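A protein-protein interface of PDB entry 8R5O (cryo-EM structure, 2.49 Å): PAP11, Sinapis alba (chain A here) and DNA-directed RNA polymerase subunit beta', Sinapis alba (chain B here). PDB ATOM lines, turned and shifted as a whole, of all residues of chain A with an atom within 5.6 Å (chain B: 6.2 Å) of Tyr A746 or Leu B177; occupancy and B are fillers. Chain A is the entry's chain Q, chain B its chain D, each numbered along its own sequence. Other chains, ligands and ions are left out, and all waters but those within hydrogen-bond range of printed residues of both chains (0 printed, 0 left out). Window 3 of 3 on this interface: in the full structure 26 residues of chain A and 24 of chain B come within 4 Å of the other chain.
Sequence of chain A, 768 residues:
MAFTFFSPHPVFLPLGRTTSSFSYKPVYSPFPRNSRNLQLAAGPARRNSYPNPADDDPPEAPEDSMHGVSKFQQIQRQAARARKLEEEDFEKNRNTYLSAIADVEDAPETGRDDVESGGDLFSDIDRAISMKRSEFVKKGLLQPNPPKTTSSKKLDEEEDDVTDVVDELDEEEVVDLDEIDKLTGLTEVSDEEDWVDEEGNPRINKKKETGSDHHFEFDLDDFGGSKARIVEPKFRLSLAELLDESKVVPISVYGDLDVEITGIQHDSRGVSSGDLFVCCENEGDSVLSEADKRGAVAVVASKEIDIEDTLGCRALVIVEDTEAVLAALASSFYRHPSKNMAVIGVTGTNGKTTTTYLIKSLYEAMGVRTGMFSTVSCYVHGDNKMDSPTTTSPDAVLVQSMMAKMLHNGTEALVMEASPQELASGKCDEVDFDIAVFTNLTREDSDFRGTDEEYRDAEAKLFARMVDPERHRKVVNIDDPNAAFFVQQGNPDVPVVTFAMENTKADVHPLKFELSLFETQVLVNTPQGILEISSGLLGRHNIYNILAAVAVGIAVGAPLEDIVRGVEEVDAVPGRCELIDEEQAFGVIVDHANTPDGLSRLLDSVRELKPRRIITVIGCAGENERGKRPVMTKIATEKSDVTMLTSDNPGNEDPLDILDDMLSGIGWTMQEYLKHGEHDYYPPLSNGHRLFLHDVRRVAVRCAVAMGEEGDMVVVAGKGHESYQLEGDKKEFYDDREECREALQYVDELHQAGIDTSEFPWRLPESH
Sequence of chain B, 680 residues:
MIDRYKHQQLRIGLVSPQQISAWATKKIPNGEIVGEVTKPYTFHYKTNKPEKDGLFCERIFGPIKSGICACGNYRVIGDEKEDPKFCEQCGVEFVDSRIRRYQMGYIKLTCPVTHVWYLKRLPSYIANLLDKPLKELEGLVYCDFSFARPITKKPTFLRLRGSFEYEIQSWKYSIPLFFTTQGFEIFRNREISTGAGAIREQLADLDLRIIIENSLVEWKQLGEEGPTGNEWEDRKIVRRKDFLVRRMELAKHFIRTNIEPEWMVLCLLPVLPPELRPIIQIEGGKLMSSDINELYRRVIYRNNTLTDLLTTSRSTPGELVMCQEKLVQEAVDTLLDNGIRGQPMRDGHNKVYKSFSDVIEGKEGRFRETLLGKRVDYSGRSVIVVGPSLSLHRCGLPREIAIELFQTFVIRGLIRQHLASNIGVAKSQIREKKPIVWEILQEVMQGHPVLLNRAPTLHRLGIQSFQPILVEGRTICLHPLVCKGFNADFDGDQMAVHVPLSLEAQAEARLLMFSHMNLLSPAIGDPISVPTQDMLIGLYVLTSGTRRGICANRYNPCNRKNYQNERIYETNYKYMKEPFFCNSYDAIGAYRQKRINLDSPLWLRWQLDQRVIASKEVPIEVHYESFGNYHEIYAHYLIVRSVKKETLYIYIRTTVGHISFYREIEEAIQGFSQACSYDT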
ATOM      1  N   ARG A 702      11.593 -14.703  24.654  1.00  0.00           N
ATOM      2  CA  ARG A 702      10.725 -13.553  24.433  1.00  0.00           C
ATOM      3  C   ARG A 702       9.406 -13.951  23.786  1.00  0.00           C
ATOM      4  O   ARG A 702       8.374 -13.331  24.060  1.00  0.00           O
ATOM      5  CB  ARG A 702      11.444 -12.507  23.587  1.00  0.00           C
ATOM      6  CG  ARG A 702      12.750 -12.040  24.193  1.00  0.00           C
ATOM      7  CD  ARG A 702      13.232 -10.755  23.559  1.00  0.00           C
ATOM      8  NE  ARG A 702      14.480 -10.303  24.156  1.00  0.00           N
ATOM      9  CZ  ARG A 702      14.980  -9.083  24.015  1.00  0.00           C
ATOM     10  NH1 ARG A 702      14.352  -8.157  23.311  1.00  0.00           N
ATOM     11  NH2 ARG A 702      16.137  -8.785  24.599  1.00  0.00           N
ATOM     12  N   GLU A 742      13.240  -7.086  29.150  1.00  0.00           N
ATOM     13  CA  GLU A 742      13.106  -6.281  27.942  1.00  0.00           C
ATOM     14  C   GLU A 742      11.919  -6.709  27.090  1.00  0.00           C
ATOM     15  O   GLU A 742      11.317  -5.868  26.414  1.00  0.00           O
ATOM     16  CB  GLU A 742      14.398  -6.349  27.128  1.00  0.00           C
ATOM     17  CG  GLU A 742      15.599  -5.738  27.836  1.00  0.00           C
ATOM     18  CD  GLU A 742      16.910  -6.038  27.138  1.00  0.00           C
ATOM     19  OE1 GLU A 742      16.890  -6.748  26.111  1.00  0.00           O
ATOM     20  OE2 GLU A 742      17.960  -5.565  27.617  1.00  0.00           O
ATOM     21  N   ALA A 743      11.567  -7.997  27.103  1.00  0.00           N
ATOM     22  CA  ALA A 743      10.412  -8.450  26.337  1.00  0.00           C
ATOM     23  C   ALA A 743       9.108  -7.912  26.910  1.00  0.00           C
ATOM     24  O   ALA A 743       8.168  -7.640  26.156  1.00  0.00           O
ATOM     25  CB  ALA A 743      10.375  -9.976  26.284  1.00  0.00           C
ATOM     26  N   LEU A 744       9.032  -7.759  28.233  1.00  0.00           N
ATOM     27  CA  LEU A 744       7.831  -7.208  28.852  1.00  0.00           C
ATOM     28  C   LEU A 744       7.615  -5.751  28.467  1.00  0.00           C
ATOM     29  O   LEU A 744       6.468  -5.315  28.319  1.00  0.00           O
ATOM     30  CB  LEU A 744       7.916  -7.345  30.372  1.00  0.00           C
ATOM     31  CG  LEU A 744       7.748  -8.749  30.951  1.00  0.00           C
ATOM     32  CD1 LEU A 744       8.236  -8.794  32.387  1.00  0.00           C
ATOM     33  CD2 LEU A 744       6.295  -9.181  30.870  1.00  0.00           C
ATOM     34  N   GLN A 745       8.696  -4.983  28.312  1.00  0.00           N
ATOM     35  CA  GLN A 745       8.562  -3.575  27.957  1.00  0.00           C
ATOM     36  C   GLN A 745       7.969  -3.399  26.565  1.00  0.00           C
ATOM     37  O   GLN A 745       7.105  -2.539  26.359  1.00  0.00           O
ATOM     38  CB  GLN A 745       9.920  -2.880  28.047  1.00  0.00           C
ATOM     39  CG  GLN A 745      10.544  -2.916  29.431  1.00  0.00           C
ATOM     40  CD  GLN A 745      11.919  -2.282  29.465  1.00  0.00           C
ATOM     41  OE1 GLN A 745      12.412  -1.784  28.452  1.00  0.00           O
ATOM     42  NE2 GLN A 745      12.549  -2.297  30.634  1.00  0.00           N
ATOM     43  N   TYR A 746       8.413  -4.200  25.598  1.00  0.00           N
ATOM     44  CA  TYR A 746       8.051  -4.010  24.201  1.00  0.00           C
ATOM     45  C   TYR A 746       6.948  -4.948  23.728  1.00  0.00           C
ATOM     46  O   TYR A 746       6.671  -5.001  22.526  1.00  0.00           O
ATOM     47  CB  TYR A 746       9.286  -4.172  23.313  1.00  0.00           C
ATOM     48  CG  TYR A 746      10.419  -3.239  23.670  1.00  0.00           C
ATOM     49  CD1 TYR A 746      10.298  -1.869  23.483  1.00  0.00           C
ATOM     50  CD2 TYR A 746      11.610  -3.726  24.185  1.00  0.00           C
ATOM     51  CE1 TYR A 746      11.331  -1.011  23.808  1.00  0.00           C
ATOM     52  CE2 TYR A 746      12.649  -2.876  24.511  1.00  0.00           C
ATOM     53  CZ  TYR A 746      12.503  -1.520  24.321  1.00  0.00           C
ATOM     54  OH  TYR A 746      13.535  -0.669  24.644  1.00  0.00           O
ATOM     55  N   VAL A 747       6.315  -5.694  24.636  1.00  0.00           N
ATOM     56  CA  VAL A 747       5.219  -6.561  24.221  1.00  0.00           C
ATOM     57  C   VAL A 747       3.968  -5.756  23.896  1.00  0.00           C
ATOM     58  O   VAL A 747       3.115  -6.223  23.130  1.00  0.00           O
ATOM     59  CB  VAL A 747       4.934  -7.623  25.301  1.00  0.00           C
ATOM     60  CG1 VAL A 747       4.281  -6.992  26.524  1.00  0.00           C
ATOM     61  CG2 VAL A 747       4.073  -8.747  24.740  1.00  0.00           C
ATOM     62  N   ASP A 748       3.838  -4.548  24.449  1.00  0.00           N
ATOM     63  CA  ASP A 748       2.655  -3.732  24.191  1.00  0.00           C
ATOM     64  C   ASP A 748       2.612  -3.258  22.742  1.00  0.00           C
ATOM     65  O   ASP A 748       1.579  -3.372  22.073  1.00  0.00           O
ATOM     66  CB  ASP A 748       2.620  -2.544  25.153  1.00  0.00           C
ATOM     67  CG  ASP A 748       3.887  -1.711  25.098  1.00  0.00           C
ATOM     68  OD1 ASP A 748       4.922  -2.237  24.638  1.00  0.00           O
ATOM     69  OD2 ASP A 748       3.847  -0.535  25.513  1.00  0.00           O
ATOM     70  N   GLU A 749       3.728  -2.722  22.240  1.00  0.00           N
ATOM     71  CA  GLU A 749       3.766  -2.231  20.869  1.00  0.00           C
ATOM     72  C   GLU A 749       3.622  -3.350  19.848  1.00  0.00           C
ATOM     73  O   GLU A 749       3.194  -3.091  18.718  1.00  0.00           O
ATOM     74  CB  GLU A 749       5.063  -1.453  20.626  1.00  0.00           C
ATOM     75  CG  GLU A 749       6.336  -2.232  20.917  1.00  0.00           C
ATOM     76  CD  GLU A 749       6.813  -3.045  19.729  1.00  0.00           C
ATOM     77  OE1 GLU A 749       6.385  -2.749  18.594  1.00  0.00           O
ATOM     78  OE2 GLU A 749       7.614  -3.982  19.930  1.00  0.00           O
ATOM     79  N   LEU A 750       3.974  -4.582  20.218  1.00  0.00           N
ATOM     80  CA  LEU A 750       3.809  -5.708  19.306  1.00  0.00           C
ATOM     81  C   LEU A 750       2.339  -6.062  19.123  1.00  0.00           C
ATOM     82  O   LEU A 750       1.912  -6.416  18.018  1.00  0.00           O
ATOM     83  CB  LEU A 750       4.592  -6.913  19.826  1.00  0.00           C
ATOM     84  CG  LEU A 750       4.979  -8.003  18.828  1.00  0.00           C
ATOM     85  CD1 LEU A 750       6.145  -7.545  17.970  1.00  0.00           C
ATOM     86  CD2 LEU A 750       5.317  -9.288  19.558  1.00  0.00           C
ATOM     87  N   LYS B 172       9.239  -4.000   9.884  1.00  0.00           N
ATOM     88  CA  LYS B 172      10.169  -2.883   9.788  1.00  0.00           C
ATOM     89  C   LYS B 172      10.495  -2.271  11.146  1.00  0.00           C
ATOM     90  O   LYS B 172      11.646  -1.893  11.390  1.00  0.00           O
ATOM     91  CB  LYS B 172       9.596  -1.817   8.849  1.00  0.00           C
ATOM     92  CG  LYS B 172      10.510  -0.633   8.597  1.00  0.00           C
ATOM     93  CD  LYS B 172      10.090   0.120   7.344  1.00  0.00           C
ATOM     94  CE  LYS B 172       8.600   0.423   7.352  1.00  0.00           C
ATOM     95  NZ  LYS B 172       8.152   1.090   6.099  1.00  0.00           N
ATOM     96  N   TYR B 173       9.511  -2.164  12.040  1.00  0.00           N
ATOM     97  CA  TYR B 173       9.724  -1.533  13.336  1.00  0.00           C
ATOM     98  C   TYR B 173       9.482  -2.469  14.510  1.00  0.00           C
ATOM     99  O   TYR B 173      10.359  -2.609  15.371  1.00  0.00           O
ATOM    100  CB  TYR B 173       8.823  -0.294  13.474  1.00  0.00           C
ATOM    101  CG  TYR B 173       8.940   0.679  12.326  1.00  0.00           C
ATOM    102  CD1 TYR B 173      10.143   1.320  12.053  1.00  0.00           C
ATOM    103  CD2 TYR B 173       7.848   0.965  11.519  1.00  0.00           C
ATOM    104  CE1 TYR B 173      10.254   2.212  11.004  1.00  0.00           C
ATOM    105  CE2 TYR B 173       7.948   1.856  10.470  1.00  0.00           C
ATOM    106  CZ  TYR B 173       9.154   2.476  10.215  1.00  0.00           C
ATOM    107  OH  TYR B 173       9.258   3.364   9.169  1.00  0.00           O
ATOM    108  N   SER B 174       8.314  -3.111  14.573  1.00  0.00           N
ATOM    109  CA  SER B 174       7.916  -3.819  15.787  1.00  0.00           C
ATOM    110  C   SER B 174       8.818  -5.016  16.069  1.00  0.00           C
ATOM    111  O   SER B 174       9.359  -5.148  17.173  1.00  0.00           O
ATOM    112  CB  SER B 174       6.457  -4.260  15.675  1.00  0.00           C
ATOM    113  OG  SER B 174       5.603  -3.143  15.508  1.00  0.00           O
ATOM    114  N   ILE B 175       8.986  -5.905  15.086  1.00  0.00           N
ATOM    115  CA  ILE B 175       9.766  -7.123  15.318  1.00  0.00           C
ATOM    116  C   ILE B 175      11.234  -6.828  15.611  1.00  0.00           C
ATOM    117  O   ILE B 175      11.776  -7.404  16.567  1.00  0.00           O
ATOM    118  CB  ILE B 175       9.573  -8.107  14.149  1.00  0.00           C
ATOM    119  CG1 ILE B 175       8.178  -8.731  14.194  1.00  0.00           C
ATOM    120  CG2 ILE B 175      10.609  -9.207  14.204  1.00  0.00           C
ATOM    121  CD1 ILE B 175       7.149  -8.002  13.376  1.00  0.00           C
ATOM    122  N   PRO B 176      11.934  -5.976  14.849  1.00  0.00           N
ATOM    123  CA  PRO B 176      13.327  -5.670  15.219  1.00  0.00           C
ATOM    124  C   PRO B 176      13.466  -5.041  16.593  1.00  0.00           C
ATOM    125  O   PRO B 176      14.478  -5.263  17.266  1.00  0.00           O
ATOM    126  CB  PRO B 176      13.782  -4.709  14.111  1.00  0.00           C
ATOM    127  CG  PRO B 176      12.900  -5.016  12.964  1.00  0.00           C
ATOM    128  CD  PRO B 176      11.572  -5.347  13.565  1.00  0.00           C
ATOM    129  N   LEU B 177      12.479  -4.256  17.027  1.00  0.00           N
ATOM    130  CA  LEU B 177      12.542  -3.651  18.353  1.00  0.00           C
ATOM    131  C   LEU B 177      12.293  -4.684  19.445  1.00  0.00           C
ATOM    132  O   LEU B 177      12.946  -4.656  20.495  1.00  0.00           O
ATOM    133  CB  LEU B 177      11.525  -2.514  18.453  1.00  0.00           C
ATOM    134  CG  LEU B 177      11.344  -1.837  19.811  1.00  0.00           C
ATOM    135  CD1 LEU B 177      12.454  -0.831  20.076  1.00  0.00           C
ATOM    136  CD2 LEU B 177       9.977  -1.176  19.903  1.00  0.00           C
ATOM    137  N   PHE B 178      11.350  -5.600  19.216  1.00  0.00           N
ATOM    138  CA  PHE B 178      10.981  -6.567  20.244  1.00  0.00           C
ATOM    139  C   PHE B 178      12.113  -7.546  20.531  1.00  0.00           C
ATOM    140  O   PHE B 178      12.376  -7.874  21.693  1.00  0.00           O
ATOM    141  CB  PHE B 178       9.717  -7.313  19.822  1.00  0.00           C
ATOM    142  CG  PHE B 178       9.244  -8.319  20.825  1.00  0.00           C
ATOM    143  CD1 PHE B 178       8.617  -7.912  21.990  1.00  0.00           C
ATOM    144  CD2 PHE B 178       9.415  -9.673  20.599  1.00  0.00           C
ATOM    145  CE1 PHE B 178       8.178  -8.837  22.913  1.00  0.00           C
ATOM    146  CE2 PHE B 178       8.977 -10.601  21.517  1.00  0.00           C
ATOM    147  CZ  PHE B 178       8.358 -10.184  22.676  1.00  0.00           C
ATOM    148  N   PHE B 179      12.791  -8.025  19.491  1.00  0.00           N
ATOM    149  CA  PHE B 179      13.876  -8.985  19.645  1.00  0.00           C
ATOM    150  C   PHE B 179      15.249  -8.332  19.708  1.00  0.00           C
ATOM    151  O   PHE B 179      16.249  -9.051  19.810  1.00  0.00           O
ATOM    152  CB  PHE B 179      13.858  -9.998  18.495  1.00  0.00           C
ATOM    153  CG  PHE B 179      12.661 -10.906  18.497  1.00  0.00           C
ATOM    154  CD1 PHE B 179      12.601 -11.991  19.352  1.00  0.00           C
ATOM    155  CD2 PHE B 179      11.608 -10.685  17.626  1.00  0.00           C
ATOM    156  CE1 PHE B 179      11.506 -12.830  19.350  1.00  0.00           C
ATOM    157  CE2 PHE B 179      10.512 -11.522  17.620  1.00  0.00           C
ATOM    158  CZ  PHE B 179      10.461 -12.596  18.482  1.00  0.00           C
ATOM    159  N   THR B 180      15.316  -6.998  19.637  1.00  0.00           N
ATOM    160  CA  THR B 180      16.550  -6.218  19.538  1.00  0.00           C
ATOM    161  C   THR B 180      17.237  -6.471  18.201  1.00  0.00           C
ATOM    162  O   THR B 180      17.135  -7.565  17.638  1.00  0.00           O
ATOM    163  CB  THR B 180      17.515  -6.503  20.697  1.00  0.00           C
ATOM    164  OG1 THR B 180      18.007  -7.846  20.606  1.00  0.00           O
ATOM    165  CG2 THR B 180      16.818  -6.307  22.034  1.00  0.00           C
ATOM    166  N   THR B 181      17.944  -5.463  17.685  1.00  0.00           N
ATOM    167  CA  THR B 181      18.532  -5.575  16.353  1.00  0.00           C
ATOM    168  C   THR B 181      19.597  -6.663  16.297  1.00  0.00           C
ATOM    169  O   THR B 181      19.669  -7.415  15.319  1.00  0.00           O
ATOM    170  CB  THR B 181      19.116  -4.231  15.921  1.00  0.00           C
ATOM    171  OG1 THR B 181      20.097  -3.805  16.875  1.00  0.00           O
ATOM    172  CG2 THR B 181      18.020  -3.181  15.825  1.00  0.00           C
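Among the printed residues, merely in contact across the chains: Arg A702 with Thr B180, Ala A743 with Phe B178, Tyr A746 with Phe B178, Tyr A746 with Leu B177, Glu A749 with Leu B177, Arg A702 with Phe B179, Glu A749 with Phe B178 and Val A747 with Phe B178.
The guanidinium group (NH2) of Arg A702 lies within salt-bridge range of the side-chain carboxylate (OE1) of Glu A742, at 2.6 Å.
Tyr A746 touches just these residues of chain B: Leu B177 and Phe B178.
Leu B177 touches two residues of chain A.
Printed residues of chain B within 4 Å of Arg A702: Phe B178 (2.6 Å), Phe B179 (3.7 Å) and Thr B180 (3.3 Å).
Of the printed residues of chain B, Glu A749 touches Ser B174 (3.2 Å), Leu B177 (3.7 Å) and Phe B178 (3.9 Å).
Printed residues of chain B within 4 Å of Ala A743: Phe B178.
Asp A748 touches none of the printed residues of chain B.
The nearest residue of chain B that does not touch Tyr A746 is Thr B180 (5.9 Å).
The nearest residue of chain A that does not touch Leu B177 is Arg A702 (4.7 Å).
Of the 10 printed residues of chain B, 5 touch a printed residue of chain A.
Among the printed residues, 10 pairs touch across the chains.
Among the printed residues, no Asp or Glu carboxylate lies within 4 Å of a Lys or Arg side-chain nitrogen of the other chain.
O of Phe B178 lies within hydrogen-bond range of NH1 of Arg A702 (2.6 Å).
The side-chain hydroxyl of Ser B174 sits at hydrogen-bond distance from the side-chain carboxylate of Glu A749, at 3.2 Å.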
